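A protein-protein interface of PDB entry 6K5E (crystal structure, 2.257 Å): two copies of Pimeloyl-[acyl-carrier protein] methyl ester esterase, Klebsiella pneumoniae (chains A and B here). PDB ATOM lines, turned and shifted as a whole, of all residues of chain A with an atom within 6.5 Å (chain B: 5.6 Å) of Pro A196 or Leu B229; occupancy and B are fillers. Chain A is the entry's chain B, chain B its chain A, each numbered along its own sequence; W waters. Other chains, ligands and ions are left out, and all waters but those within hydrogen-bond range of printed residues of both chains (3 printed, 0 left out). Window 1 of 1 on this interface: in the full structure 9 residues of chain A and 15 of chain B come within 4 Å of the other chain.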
ATOM      1  N   ALA A  92      14.260  -2.727  -8.101  1.00  0.00           N
ATOM      2  CA  ALA A  92      14.136  -1.378  -8.640  1.00  0.00           C
ATOM      3  C   ALA A  92      12.680  -0.965  -8.725  1.00  0.00           C
ATOM      4  O   ALA A  92      12.297   0.114  -8.264  1.00  0.00           O
ATOM      5  CB  ALA A  92      14.774  -1.293 -10.019  1.00  0.00           C
ATOM      6  N   PRO A  96      11.982   1.757  -5.501  1.00  0.00           N
ATOM      7  CA  PRO A  96      12.945   2.687  -6.129  1.00  0.00           C
ATOM      8  C   PRO A  96      13.730   3.533  -5.130  1.00  0.00           C
ATOM      9  O   PRO A  96      14.870   3.916  -5.418  1.00  0.00           O
ATOM     10  CB  PRO A  96      12.061   3.559  -7.039  1.00  0.00           C
ATOM     11  CG  PRO A  96      10.645   3.368  -6.560  1.00  0.00           C
ATOM     12  CD  PRO A  96      10.605   1.962  -6.000  1.00  0.00           C
ATOM     13  N   GLN A 100      19.851   3.321  -5.885  1.00  0.00           N
ATOM     14  CA  GLN A 100      20.463   4.520  -6.452  1.00  0.00           C
ATOM     15  C   GLN A 100      20.550   4.434  -7.971  1.00  0.00           C
ATOM     16  O   GLN A 100      20.425   5.456  -8.662  1.00  0.00           O
ATOM     17  CB  GLN A 100      21.851   4.736  -5.844  1.00  0.00           C
ATOM     18  CG  GLN A 100      21.812   4.876  -4.319  1.00  0.00           C
ATOM     19  CD  GLN A 100      23.094   5.480  -3.729  1.00  0.00           C
ATOM     20  OE1 GLN A 100      24.199   5.231  -4.215  1.00  0.00           O
ATOM     21  NE2 GLN A 100      22.940   6.290  -2.680  1.00  0.00           N
ATOM     22  N   VAL A 193      10.107   0.337 -18.139  1.00  0.00           N
ATOM     23  CA  VAL A 193      10.018   1.556 -18.929  1.00  0.00           C
ATOM     24  C   VAL A 193      10.051   2.800 -18.031  1.00  0.00           C
ATOM     25  O   VAL A 193      10.714   3.795 -18.343  1.00  0.00           O
ATOM     26  CB  VAL A 193       8.744   1.487 -19.800  1.00  0.00           C
ATOM     27  CG1 VAL A 193       8.385   2.838 -20.371  1.00  0.00           C
ATOM     28  CG2 VAL A 193       8.930   0.456 -20.928  1.00  0.00           C
ATOM     29  N   ARG A 194       9.356   2.758 -16.896  1.00  0.00           N
ATOM     30  CA  ARG A 194       9.101   3.942 -16.084  1.00  0.00           C
ATOM     31  C   ARG A 194      10.027   4.041 -14.879  1.00  0.00           C
ATOM     32  O   ARG A 194       9.664   4.655 -13.870  1.00  0.00           O
ATOM     33  CB  ARG A 194       7.641   3.970 -15.629  1.00  0.00           C
ATOM     34  CG  ARG A 194       6.621   3.973 -16.783  1.00  0.00           C
ATOM     35  CD  ARG A 194       6.908   5.066 -17.831  1.00  0.00           C
ATOM     36  NE  ARG A 194       6.068   4.920 -19.030  1.00  0.00           N
ATOM     37  CZ  ARG A 194       6.161   5.692 -20.116  1.00  0.00           C
ATOM     38  NH1 ARG A 194       7.060   6.675 -20.164  1.00  0.00           N
ATOM     39  NH2 ARG A 194       5.363   5.481 -21.163  1.00  0.00           N
ATOM     40  N   LEU A 195      11.206   3.444 -14.960  1.00  0.00           N
ATOM     41  CA  LEU A 195      12.170   3.523 -13.869  1.00  0.00           C
ATOM     42  C   LEU A 195      12.680   4.960 -13.707  1.00  0.00           C
ATOM     43  O   LEU A 195      12.988   5.638 -14.700  1.00  0.00           O
ATOM     44  CB  LEU A 195      13.343   2.594 -14.144  1.00  0.00           C
ATOM     45  CG  LEU A 195      13.353   1.136 -13.713  1.00  0.00           C
ATOM     46  CD1 LEU A 195      14.799   0.737 -13.646  1.00  0.00           C
ATOM     47  CD2 LEU A 195      12.683   0.930 -12.363  1.00  0.00           C
ATOM     48  N   PRO A 196      12.812   5.451 -12.466  1.00  0.00           N
ATOM     49  CA  PRO A 196      13.204   6.849 -12.275  1.00  0.00           C
ATOM     50  C   PRO A 196      14.713   7.075 -12.207  1.00  0.00           C
ATOM     51  O   PRO A 196      15.179   8.189 -12.476  1.00  0.00           O
ATOM     52  CB  PRO A 196      12.526   7.203 -10.950  1.00  0.00           C
ATOM     53  CG  PRO A 196      12.514   5.904 -10.194  1.00  0.00           C
ATOM     54  CD  PRO A 196      12.444   4.800 -11.195  1.00  0.00           C
ATOM     55  N   MET A 197      15.471   6.040 -11.860  1.00  0.00           N
ATOM     56  CA  MET A 197      16.904   6.092 -11.608  1.00  0.00           C
ATOM     57  C   MET A 197      17.718   5.609 -12.823  1.00  0.00           C
ATOM     58  O   MET A 197      17.175   5.062 -13.790  1.00  0.00           O
ATOM     59  CB  MET A 197      17.228   5.251 -10.371  1.00  0.00           C
ATOM     60  CG  MET A 197      17.281   3.772 -10.666  1.00  0.00           C
ATOM     61  SD  MET A 197      15.657   3.013 -10.729  1.00  0.00           S
ATOM     62  CE  MET A 197      15.205   3.162  -9.011  1.00  0.00           C
ATOM     63  N   PRO A 198      19.040   5.834 -12.818  1.00  0.00           N
ATOM     64  CA  PRO A 198      19.872   5.358 -13.932  1.00  0.00           C
ATOM     65  C   PRO A 198      19.817   3.843 -14.066  1.00  0.00           C
ATOM     66  O   PRO A 198      19.700   3.120 -13.073  1.00  0.00           O
ATOM     67  CB  PRO A 198      21.279   5.836 -13.547  1.00  0.00           C
ATOM     68  CG  PRO A 198      21.038   7.050 -12.779  1.00  0.00           C
ATOM     69  CD  PRO A 198      19.814   6.729 -11.935  1.00  0.00           C
ATOM     70  N   GLU A 224      15.642   5.775 -21.710  1.00  0.00           N
ATOM     71  CA  GLU A 224      16.433   6.426 -20.669  1.00  0.00           C
ATOM     72  C   GLU A 224      17.569   5.566 -20.120  1.00  0.00           C
ATOM     73  O   GLU A 224      18.399   6.099 -19.381  1.00  0.00           O
ATOM     74  CB  GLU A 224      15.549   6.826 -19.494  1.00  0.00           C
ATOM     75  CG  GLU A 224      14.489   7.846 -19.814  1.00  0.00           C
ATOM     76  CD  GLU A 224      13.471   7.981 -18.675  1.00  0.00           C
ATOM     77  OE1 GLU A 224      12.778   6.977 -18.344  1.00  0.00           O
ATOM     78  OE2 GLU A 224      13.384   9.089 -18.105  1.00  0.00           O
ATOM     79  N   LEU A 256      26.458   9.430 -10.790  1.00  0.00           N
ATOM     80  CA  LEU A 256      25.693   9.606  -9.558  1.00  0.00           C
ATOM     81  C   LEU A 256      26.285  10.688  -8.673  1.00  0.00           C
ATOM     82  O   LEU A 256      25.543  11.387  -7.971  1.00  0.00           O
ATOM     83  CB  LEU A 256      25.643   8.305  -8.781  1.00  0.00           C
ATOM     84  CG  LEU A 256      24.666   7.291  -9.368  1.00  0.00           C
ATOM     85  CD1 LEU A 256      25.125   5.873  -8.979  1.00  0.00           C
ATOM     86  CD2 LEU A 256      23.231   7.576  -8.924  1.00  0.00           C
ATOM     87  N   ARG B 201      10.451  12.085  -0.245  1.00  0.00           N
ATOM     88  CA  ARG B 201      10.943  13.255  -0.974  1.00  0.00           C
ATOM     89  C   ARG B 201      11.292  12.861  -2.402  1.00  0.00           C
ATOM     90  O   ARG B 201      12.123  11.974  -2.617  1.00  0.00           O
ATOM     91  CB  ARG B 201      12.162  13.877  -0.280  1.00  0.00           C
ATOM     92  CG  ARG B 201      11.985  14.173   1.199  1.00  0.00           C
ATOM     93  CD  ARG B 201      13.234  13.766   1.978  1.00  0.00           C
ATOM     94  NE  ARG B 201      14.448  14.153   1.250  1.00  0.00           N
ATOM     95  CZ  ARG B 201      15.593  13.475   1.288  1.00  0.00           C
ATOM     96  NH1 ARG B 201      15.692  12.384   2.028  1.00  0.00           N
ATOM     97  NH2 ARG B 201      16.635  13.890   0.585  1.00  0.00           N
ATOM     98  N   TYR B 203      12.642  14.254  -6.208  1.00  0.00           N
ATOM     99  CA  TYR B 203      13.484  15.291  -6.792  1.00  0.00           C
ATOM    100  C   TYR B 203      13.675  15.036  -8.278  1.00  0.00           C
ATOM    101  O   TYR B 203      13.547  13.901  -8.749  1.00  0.00           O
ATOM    102  CB  TYR B 203      14.880  15.354  -6.136  1.00  0.00           C
ATOM    103  CG  TYR B 203      14.872  15.599  -4.651  1.00  0.00           C
ATOM    104  CD1 TYR B 203      14.837  14.536  -3.761  1.00  0.00           C
ATOM    105  CD2 TYR B 203      14.912  16.897  -4.135  1.00  0.00           C
ATOM    106  CE1 TYR B 203      14.833  14.749  -2.388  1.00  0.00           C
ATOM    107  CE2 TYR B 203      14.905  17.128  -2.758  1.00  0.00           C
ATOM    108  CZ  TYR B 203      14.863  16.041  -1.890  1.00  0.00           C
ATOM    109  OH  TYR B 203      14.839  16.223  -0.524  1.00  0.00           O
ATOM    110  N   GLY B 204      13.995  16.113  -9.000  1.00  0.00           N
ATOM    111  CA  GLY B 204      14.520  16.047 -10.364  1.00  0.00           C
ATOM    112  C   GLY B 204      16.003  16.383 -10.421  1.00  0.00           C
ATOM    113  O   GLY B 204      16.459  17.342  -9.788  1.00  0.00           O
ATOM    114  N   ARG B 205      16.751  15.595 -11.206  1.00  0.00           N
ATOM    115  CA  ARG B 205      18.208  15.710 -11.241  1.00  0.00           C
ATOM    116  C   ARG B 205      18.655  17.016 -11.877  1.00  0.00           C
ATOM    117  O   ARG B 205      19.660  17.611 -11.457  1.00  0.00           O
ATOM    118  CB  ARG B 205      18.816  14.538 -12.012  1.00  0.00           C
ATOM    119  CG  ARG B 205      20.342  14.521 -11.965  1.00  0.00           C
ATOM    120  CD  ARG B 205      20.955  14.023 -13.267  1.00  0.00           C
ATOM    121  NE  ARG B 205      22.212  14.717 -13.510  1.00  0.00           N
ATOM    122  CZ  ARG B 205      23.398  14.302 -13.071  1.00  0.00           C
ATOM    123  NH1 ARG B 205      23.508  13.172 -12.364  1.00  0.00           N
ATOM    124  NH2 ARG B 205      24.484  15.025 -13.340  1.00  0.00           N
ATOM    125  N   ARG B 212      20.201  19.176  -6.583  1.00  0.00           N
ATOM    126  CA  ARG B 212      20.309  17.804  -6.133  1.00  0.00           C
ATOM    127  C   ARG B 212      21.431  17.626  -5.119  1.00  0.00           C
ATOM    128  O   ARG B 212      21.435  16.632  -4.404  1.00  0.00           O
ATOM    129  CB  ARG B 212      20.540  16.879  -7.312  1.00  0.00           C
ATOM    130  CG  ARG B 212      21.731  17.289  -8.131  1.00  0.00           C
ATOM    131  CD  ARG B 212      22.101  16.283  -9.201  1.00  0.00           C
ATOM    132  NE  ARG B 212      23.347  16.691  -9.847  1.00  0.00           N
ATOM    133  CZ  ARG B 212      24.418  15.913  -9.970  1.00  0.00           C
ATOM    134  NH1 ARG B 212      25.513  16.375 -10.568  1.00  0.00           N
ATOM    135  NH2 ARG B 212      24.400  14.676  -9.485  1.00  0.00           N
ATOM    136  N   ILE B 214      20.091  16.653  -1.538  1.00  0.00           N
ATOM    137  CA  ILE B 214      19.367  15.383  -1.375  1.00  0.00           C
ATOM    138  C   ILE B 214      20.144  14.423  -0.502  1.00  0.00           C
ATOM    139  O   ILE B 214      19.621  13.871   0.460  1.00  0.00           O
ATOM    140  CB  ILE B 214      19.073  14.650  -2.705  1.00  0.00           C
ATOM    141  CG1 ILE B 214      18.055  15.380  -3.533  1.00  0.00           C
ATOM    142  CG2 ILE B 214      18.523  13.221  -2.447  1.00  0.00           C
ATOM    143  CD1 ILE B 214      18.306  15.250  -4.988  1.00  0.00           C
ATOM    144  N   SER B 227      13.884   9.034  -0.281  1.00  0.00           N
ATOM    145  CA  SER B 227      14.058   9.979  -1.363  1.00  0.00           C
ATOM    146  C   SER B 227      14.179   9.208  -2.655  1.00  0.00           C
ATOM    147  O   SER B 227      14.796   8.141  -2.702  1.00  0.00           O
ATOM    148  CB  SER B 227      15.311  10.810  -1.197  1.00  0.00           C
ATOM    149  OG  SER B 227      16.421   9.973  -1.481  1.00  0.00           O
ATOM    150  N   ILE B 228      13.617   9.780  -3.708  1.00  0.00           N
ATOM    151  CA  ILE B 228      13.802   9.274  -5.056  1.00  0.00           C
ATOM    152  C   ILE B 228      14.246  10.430  -5.911  1.00  0.00           C
ATOM    153  O   ILE B 228      13.597  11.481  -5.906  1.00  0.00           O
ATOM    154  CB  ILE B 228      12.525   8.673  -5.645  1.00  0.00           C
ATOM    155  CG1 ILE B 228      12.002   7.533  -4.761  1.00  0.00           C
ATOM    156  CG2 ILE B 228      12.809   8.253  -7.051  1.00  0.00           C
ATOM    157  CD1 ILE B 228      10.522   7.131  -5.095  1.00  0.00           C
ATOM    158  N   LEU B 229      15.329  10.224  -6.663  1.00  0.00           N
ATOM    159  CA  LEU B 229      15.870  11.210  -7.585  1.00  0.00           C
ATOM    160  C   LEU B 229      15.484  10.822  -9.016  1.00  0.00           C
ATOM    161  O   LEU B 229      15.786   9.711  -9.464  1.00  0.00           O
ATOM    162  CB  LEU B 229      17.383  11.291  -7.408  1.00  0.00           C
ATOM    163  CG  LEU B 229      18.206  12.382  -8.071  1.00  0.00           C
ATOM    164  CD1 LEU B 229      17.469  13.683  -8.054  1.00  0.00           C
ATOM    165  CD2 LEU B 229      19.507  12.520  -7.327  1.00  0.00           C
ATOM    166  N   PHE B 230      14.804  11.730  -9.727  1.00  0.00           N
ATOM    167  CA  PHE B 230      14.400  11.481 -11.109  1.00  0.00           C
ATOM    168  C   PHE B 230      15.530  11.943 -12.025  1.00  0.00           C
ATOM    169  O   PHE B 230      15.822  13.138 -12.115  1.00  0.00           O
ATOM    170  CB  PHE B 230      13.093  12.194 -11.443  1.00  0.00           C
ATOM    171  CG  PHE B 230      11.871  11.492 -10.933  1.00  0.00           C
ATOM    172  CD1 PHE B 230      11.760  11.141  -9.608  1.00  0.00           C
ATOM    173  CD2 PHE B 230      10.820  11.200 -11.779  1.00  0.00           C
ATOM    174  CE1 PHE B 230      10.638  10.487  -9.141  1.00  0.00           C
ATOM    175  CE2 PHE B 230       9.697  10.544 -11.311  1.00  0.00           C
ATOM    176  CZ  PHE B 230       9.611  10.182  -9.988  1.00  0.00           C
ATOM    177  N   ASP B 231      16.141  10.996 -12.724  1.00  0.00           N
ATOM    178  CA  ASP B 231      17.437  11.239 -13.341  1.00  0.00           C
ATOM    179  C   ASP B 231      17.325  12.143 -14.575  1.00  0.00           C
ATOM    180  O   ASP B 231      18.277  12.862 -14.904  1.00  0.00           O
ATOM    181  CB  ASP B 231      18.077   9.879 -13.657  1.00  0.00           C
ATOM    182  CG  ASP B 231      19.368   9.995 -14.432  1.00  0.00           C
ATOM    183  OD1 ASP B 231      20.351  10.536 -13.875  1.00  0.00           O
ATOM    184  OD2 ASP B 231      19.392   9.538 -15.598  1.00  0.00           O
ATOM    185  N   LYS B 232      16.167  12.156 -15.238  1.00  0.00           N
ATOM    186  CA  LYS B 232      15.989  12.923 -16.467  1.00  0.00           C
ATOM    187  C   LYS B 232      14.924  14.015 -16.350  1.00  0.00           C
ATOM    188  O   LYS B 232      14.508  14.573 -17.381  1.00  0.00           O
ATOM    189  CB  LYS B 232      15.648  11.982 -17.628  1.00  0.00           C
ATOM    190  CG  LYS B 232      16.755  10.965 -17.973  1.00  0.00           C
ATOM    191  CD  LYS B 232      17.847  11.570 -18.868  1.00  0.00           C
ATOM    192  CE  LYS B 232      18.534  10.495 -19.719  1.00  0.00           C
ATOM    193  NZ  LYS B 232      18.998   9.321 -18.910  1.00  0.00           N
ATOM    194  N   ALA B 244       6.282   7.461 -13.764  1.00  0.00           N
ATOM    195  CA  ALA B 244       7.209   7.187 -12.672  1.00  0.00           C
ATOM    196  C   ALA B 244       6.825   7.964 -11.420  1.00  0.00           C
ATOM    197  O   ALA B 244       7.047   7.489 -10.310  1.00  0.00           O
ATOM    198  CB  ALA B 244       8.636   7.517 -13.084  1.00  0.00           C
HETATM  199  O   HOH W   1       8.569   4.890 -10.971  1.00  0.00           O
HETATM  200  O   HOH W   2      13.595  10.185 -15.082  1.00  0.00           O
HETATM  201  O   HOH W   3      20.762   7.390 -19.235  1.00  0.00           O
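No position is printed for both chains.
The backbone carbonyl oxygen (O) of Pro A196 is in hydrogen-bond range of the backbone NH (N) of Asp B231 (3.0 Å).
NZ of Lys B232 is in hydrogen-bond range of O of Glu A224 (3.3 Å).
The backbone carbonyl oxygen of Leu B229 sits close to the backbone carbonyl oxygen of Pro A196, at 3.4 Å.
Among the printed residues, merely in contact across the chains: Arg A194 with Ala B244 (3.1 Å), Pro A196 with Phe B230 (3.6 Å), Pro A198 with Asp B231 (3.7 Å), Leu A256 with Arg B212 (3.8 Å) and Pro A196 with Ile B228 (3.9 Å).
Water W3 bridges NZ of Lys B232 and O of Glu A224.
Water W1 bridges the backbone carbonyl oxygen (O) of Ala B244 and the backbone carbonyl oxygen (O) of Arg A194.
Water W2 bridges the side-chain carboxylate (OE2) of Glu A224 (3.2 Å) and the backbone NH (N) of Lys B232 (3.2 Å).
Of the printed residues of chain B, Glu A224 touches Lys B232 (3.3 Å).
Arg B201 touches none of the printed residues of chain A.
Ile B214 touches none of the printed residues of chain A.
Of the printed residues of chain A, Leu B229 touches Pro A196 (3.4 Å).
Printed residues of chain A within 4 Å of Phe B230: Pro A196.
Of the printed residues of chain A, Lys B232 touches Glu A224 (3.3 Å).
Of the printed residues of chain A, Ala B244 touches Arg A194 (3.1 Å).
Printed residues of chain B that touch a printed residue of chain A: Arg B212, Ile B228, Leu B229, Phe B230, Asp B231, Lys B232 and Ala B244.
Hydrophobic or aromatic side chains of chain B within 4 Å of the printed part of chain A: Ile B228 and Ala B244.
Of the 11 printed residues of chain A, 5 touch a printed residue of chain B.
Printed residues of chain A that touch a printed residue of chain B: Arg A194, Pro A196, Pro A198, Glu A224 and Leu A256.
Among the printed residues, 8 pairs touch across the chains.
Among the printed residues, no Asp or Glu carboxylate lies within 4 Å of a Lys or Arg side-chain nitrogen of the other chain.
N of Ile B228 lies within hydrogen-bond range of O of Arg B201, 2.9 Å away.
The backbone carbonyl oxygen (O) of Ile B228 sits at hydrogen-bond distance from the backbone NH (N) of Tyr B203, 2.9 Å away.
The backbone carbonyl oxygen (O) of Tyr B203 lies within hydrogen-bond range of the backbone NH (N) of Phe B230 (2.7 Å).
O of Phe B230 is in hydrogen-bond range of N of Arg B205 (2.8 Å).
The side-chain amino group of Lys B232 is in salt-bridge range of the side-chain carboxylate of Asp B231, at 3.3 Å.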
